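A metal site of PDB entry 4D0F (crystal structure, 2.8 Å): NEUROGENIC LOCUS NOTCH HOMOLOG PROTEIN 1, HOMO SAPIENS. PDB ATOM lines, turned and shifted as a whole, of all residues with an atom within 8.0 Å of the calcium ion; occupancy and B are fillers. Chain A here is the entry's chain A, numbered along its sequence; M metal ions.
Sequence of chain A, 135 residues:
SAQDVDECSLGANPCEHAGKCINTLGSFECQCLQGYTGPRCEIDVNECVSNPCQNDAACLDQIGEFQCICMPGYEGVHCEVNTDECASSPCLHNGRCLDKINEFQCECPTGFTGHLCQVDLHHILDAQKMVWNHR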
ATOM      1  N   GLN A  34     -33.014   9.949  13.888  1.00  0.00           N
ATOM      2  CA  GLN A  34     -31.721  10.611  13.989  1.00  0.00           C
ATOM      3  C   GLN A  34     -30.641   9.820  13.284  1.00  0.00           C
ATOM      4  O   GLN A  34     -30.531   8.593  13.450  1.00  0.00           O
ATOM      5  CB  GLN A  34     -31.335  10.856  15.437  1.00  0.00           C
ATOM      6  CG  GLN A  34     -30.114  11.751  15.610  1.00  0.00           C
ATOM      7  CD  GLN A  34     -30.049  12.313  16.993  1.00  0.00           C
ATOM      8  OE1 GLN A  34     -31.077  12.678  17.589  1.00  0.00           O
ATOM      9  NE2 GLN A  34     -28.824  12.409  17.501  1.00  0.00           N
ATOM     10  N   GLY A  35     -29.886  10.538  12.459  1.00  0.00           N
ATOM     11  CA  GLY A  35     -28.785   9.982  11.693  1.00  0.00           C
ATOM     12  C   GLY A  35     -29.129   9.632  10.282  1.00  0.00           C
ATOM     13  O   GLY A  35     -28.252   9.185   9.542  1.00  0.00           O
ATOM     14  N   TYR A  36     -30.422   9.829   9.886  1.00  0.00           N
ATOM     15  CA  TYR A  36     -30.856   9.536   8.521  1.00  0.00           C
ATOM     16  C   TYR A  36     -31.413  10.760   7.847  1.00  0.00           C
ATOM     17  O   TYR A  36     -32.033  11.598   8.515  1.00  0.00           O
ATOM     18  CB  TYR A  36     -31.837   8.383   8.501  1.00  0.00           C
ATOM     19  CG  TYR A  36     -31.272   7.100   9.050  1.00  0.00           C
ATOM     20  CD1 TYR A  36     -30.392   6.320   8.286  1.00  0.00           C
ATOM     21  CD2 TYR A  36     -31.593   6.666  10.332  1.00  0.00           C
ATOM     22  CE1 TYR A  36     -29.862   5.133   8.790  1.00  0.00           C
ATOM     23  CE2 TYR A  36     -31.052   5.491  10.854  1.00  0.00           C
ATOM     24  CZ  TYR A  36     -30.186   4.719  10.071  1.00  0.00           C
ATOM     25  OH  TYR A  36     -29.689   3.537  10.570  1.00  0.00           O
ATOM     26  N   ILE A  43     -30.452   7.919   3.221  1.00  0.00           N
ATOM     27  CA  ILE A  43     -29.070   8.210   3.533  1.00  0.00           C
ATOM     28  C   ILE A  43     -28.685   8.152   4.979  1.00  0.00           C
ATOM     29  O   ILE A  43     -29.304   8.797   5.825  1.00  0.00           O
ATOM     30  CB  ILE A  43     -28.604   9.552   2.864  1.00  0.00           C
ATOM     31  CG1 ILE A  43     -29.183   9.795   1.432  1.00  0.00           C
ATOM     32  CG2 ILE A  43     -27.096   9.761   2.964  1.00  0.00           C
ATOM     33  CD1 ILE A  43     -28.896   8.758   0.288  1.00  0.00           C
ATOM     34  N   ASP A  44     -27.592   7.451   5.241  1.00  0.00           N
ATOM     35  CA  ASP A  44     -26.966   7.408   6.533  1.00  0.00           C
ATOM     36  C   ASP A  44     -25.999   8.630   6.517  1.00  0.00           C
ATOM     37  O   ASP A  44     -24.953   8.622   5.856  1.00  0.00           O
ATOM     38  CB  ASP A  44     -26.222   6.081   6.719  1.00  0.00           C
ATOM     39  CG  ASP A  44     -25.277   6.013   7.894  1.00  0.00           C
ATOM     40  OD1 ASP A  44     -25.173   7.017   8.641  1.00  0.00           O
ATOM     41  OD2 ASP A  44     -24.640   4.954   8.079  1.00  0.00           O
ATOM     42  N   VAL A  45     -26.394   9.682   7.242  1.00  0.00           N
ATOM     43  CA  VAL A  45     -25.609  10.908   7.391  1.00  0.00           C
ATOM     44  C   VAL A  45     -24.161  10.582   7.768  1.00  0.00           C
ATOM     45  O   VAL A  45     -23.924   9.695   8.606  1.00  0.00           O
ATOM     46  CB  VAL A  45     -26.226  11.877   8.445  1.00  0.00           C
ATOM     47  CG1 VAL A  45     -25.368  13.113   8.690  1.00  0.00           C
ATOM     48  CG2 VAL A  45     -27.613  12.292   8.039  1.00  0.00           C
ATOM     49  N   ASN A  46     -23.201  11.309   7.176  1.00  0.00           N
ATOM     50  CA  ASN A  46     -21.794  11.199   7.527  1.00  0.00           C
ATOM     51  C   ASN A  46     -21.529  12.205   8.676  1.00  0.00           C
ATOM     52  O   ASN A  46     -21.288  13.393   8.444  1.00  0.00           O
ATOM     53  CB  ASN A  46     -20.871  11.488   6.336  1.00  0.00           C
ATOM     54  CG  ASN A  46     -19.399  11.458   6.693  1.00  0.00           C
ATOM     55  OD1 ASN A  46     -18.989  11.041   7.785  1.00  0.00           O
ATOM     56  ND2 ASN A  46     -18.570  11.904   5.761  1.00  0.00           N
ATOM     57  N   GLU A  47     -21.554  11.704   9.916  1.00  0.00           N
ATOM     58  CA  GLU A  47     -21.364  12.537  11.103  1.00  0.00           C
ATOM     59  C   GLU A  47     -19.941  13.078  11.230  1.00  0.00           C
ATOM     60  O   GLU A  47     -19.715  13.947  12.064  1.00  0.00           O
ATOM     61  CB  GLU A  47     -21.823  11.811  12.379  1.00  0.00           C
ATOM     62  CG  GLU A  47     -23.335  11.702  12.535  1.00  0.00           C
ATOM     63  CD  GLU A  47     -23.986  10.568  11.772  1.00  0.00           C
ATOM     64  OE1 GLU A  47     -23.270   9.602  11.428  1.00  0.00           O
ATOM     65  OE2 GLU A  47     -25.178  10.689  11.423  1.00  0.00           O
ATOM     66  N   CYS A  48     -19.015  12.598  10.366  1.00  0.00           N
ATOM     67  CA  CYS A  48     -17.610  13.014  10.325  1.00  0.00           C
ATOM     68  C   CYS A  48     -17.310  14.121   9.347  1.00  0.00           C
ATOM     69  O   CYS A  48     -16.197  14.647   9.331  1.00  0.00           O
ATOM     70  CB  CYS A  48     -16.716  11.801  10.056  1.00  0.00           C
ATOM     71  SG  CYS A  48     -16.676  10.611  11.401  1.00  0.00           S
ATOM     72  N   LEU A  60     -14.882   8.049  13.304  1.00  0.00           N
ATOM     73  CA  LEU A  60     -15.679   6.893  12.881  1.00  0.00           C
ATOM     74  C   LEU A  60     -17.112   7.312  12.622  1.00  0.00           C
ATOM     75  O   LEU A  60     -17.802   7.785  13.519  1.00  0.00           O
ATOM     76  CB  LEU A  60     -15.633   5.756  13.905  1.00  0.00           C
ATOM     77  CG  LEU A  60     -14.278   5.194  14.282  1.00  0.00           C
ATOM     78  CD1 LEU A  60     -14.446   4.137  15.278  1.00  0.00           C
ATOM     79  CD2 LEU A  60     -13.518   4.650  13.065  1.00  0.00           C
ATOM     80  N   ASP A  61     -17.564   7.147  11.383  1.00  0.00           N
ATOM     81  CA  ASP A  61     -18.915   7.528  10.982  1.00  0.00           C
ATOM     82  C   ASP A  61     -19.852   6.360  11.290  1.00  0.00           C
ATOM     83  O   ASP A  61     -19.826   5.345  10.600  1.00  0.00           O
ATOM     84  CB  ASP A  61     -18.911   7.906   9.495  1.00  0.00           C
ATOM     85  CG  ASP A  61     -20.278   8.102   8.855  1.00  0.00           C
ATOM     86  OD1 ASP A  61     -21.245   8.364   9.600  1.00  0.00           O
ATOM     87  OD2 ASP A  61     -20.369   8.031   7.622  1.00  0.00           O
ATOM     88  N   GLN A  62     -20.668   6.512  12.333  1.00  0.00           N
ATOM     89  CA  GLN A  62     -21.538   5.445  12.809  1.00  0.00           C
ATOM     90  C   GLN A  62     -23.002   5.778  12.651  1.00  0.00           C
ATOM     91  O   GLN A  62     -23.330   6.763  11.999  1.00  0.00           O
ATOM     92  CB  GLN A  62     -21.183   5.120  14.253  1.00  0.00           C
ATOM     93  CG  GLN A  62     -19.699   4.799  14.434  1.00  0.00           C
ATOM     94  CD  GLN A  62     -19.292   4.734  15.881  1.00  0.00           C
ATOM     95  OE1 GLN A  62     -19.937   5.305  16.775  1.00  0.00           O
ATOM     96  NE2 GLN A  62     -18.214   4.021  16.133  1.00  0.00           N
ATOM     97  N   ILE A  63     -23.889   4.931  13.204  1.00  0.00           N
ATOM     98  CA  ILE A  63     -25.325   5.126  13.095  1.00  0.00           C
ATOM     99  C   ILE A  63     -25.782   6.230  14.029  1.00  0.00           C
ATOM    100  O   ILE A  63     -25.717   6.045  15.251  1.00  0.00           O
ATOM    101  CB  ILE A  63     -26.129   3.786  13.244  1.00  0.00           C
ATOM    102  CG1 ILE A  63     -25.562   2.678  12.299  1.00  0.00           C
ATOM    103  CG2 ILE A  63     -27.629   4.013  13.035  1.00  0.00           C
ATOM    104  CD1 ILE A  63     -25.790   1.341  12.719  1.00  0.00           C
ATOM    105  N   GLY A  64     -26.192   7.364  13.425  1.00  0.00           N
ATOM    106  CA  GLY A  64     -26.674   8.556  14.126  1.00  0.00           C
ATOM    107  C   GLY A  64     -25.684   9.213  15.065  1.00  0.00           C
ATOM    108  O   GLY A  64     -26.083   9.951  15.967  1.00  0.00           O
ATOM    109  N   GLU A  65     -24.368   8.970  14.857  1.00  0.00           N
ATOM    110  CA  GLU A  65     -23.298   9.467  15.734  1.00  0.00           C
ATOM    111  C   GLU A  65     -21.937   9.242  15.099  1.00  0.00           C
ATOM    112  O   GLU A  65     -21.777   8.479  14.136  1.00  0.00           O
ATOM    113  CB  GLU A  65     -23.358   8.607  17.007  1.00  0.00           C
ATOM    114  CG  GLU A  65     -22.976   9.216  18.323  1.00  0.00           C
ATOM    115  CD  GLU A  65     -23.010   8.127  19.376  1.00  0.00           C
ATOM    116  OE1 GLU A  65     -22.975   6.931  18.994  1.00  0.00           O
ATOM    117  OE2 GLU A  65     -23.057   8.471  20.580  1.00  0.00           O
ATOM    118  N   PHE A  66     -20.934   9.892  15.657  1.00  0.00           N
ATOM    119  CA  PHE A  66     -19.544   9.691  15.322  1.00  0.00           C
ATOM    120  C   PHE A  66     -18.848   9.264  16.587  1.00  0.00           C
ATOM    121  O   PHE A  66     -19.338   9.534  17.676  1.00  0.00           O
ATOM    122  CB  PHE A  66     -18.880  10.951  14.753  1.00  0.00           C
ATOM    123  CG  PHE A  66     -18.816  12.100  15.728  1.00  0.00           C
ATOM    124  CD1 PHE A  66     -19.860  13.009  15.826  1.00  0.00           C
ATOM    125  CD2 PHE A  66     -17.715  12.268  16.550  1.00  0.00           C
ATOM    126  CE1 PHE A  66     -19.815  14.054  16.737  1.00  0.00           C
ATOM    127  CE2 PHE A  66     -17.680  13.312  17.479  1.00  0.00           C
ATOM    128  CZ  PHE A  66     -18.720  14.201  17.555  1.00  0.00           C
HETATM  129 CA    CA M   1     -23.725   7.710  10.017  1.00  0.00          CA
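The backbone carbonyl oxygen (O) of Gly 35 lies within hydrogen-bond range of the backbone NH (N) of Val 45, 3.0 Å away.
N of Asp 61 lies within hydrogen-bond range of SG of Cys 48 (3.6 Å).
OD1 of Asn 46 sits close to OD2 of Asp 61, at 3.3 Å.
The nearest printed residue that does not touch the calcium ion is Gly 64 (4.2 Å).
The calcium ion is bound by the side-chain carboxylate (OD1) of Asp 44 (2.1 Å), the backbone carbonyl oxygen (O) of Gln 62 (2.2 Å), the side-chain carboxylate (OE1) of Glu 47 (2.4 Å), the backbone carbonyl oxygen (O) of Val 45 (2.4 Å) and the side-chain carboxylate (OD1) of Asp 61 (2.6 Å).
The calcium ion has five donor atoms within binding distance.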
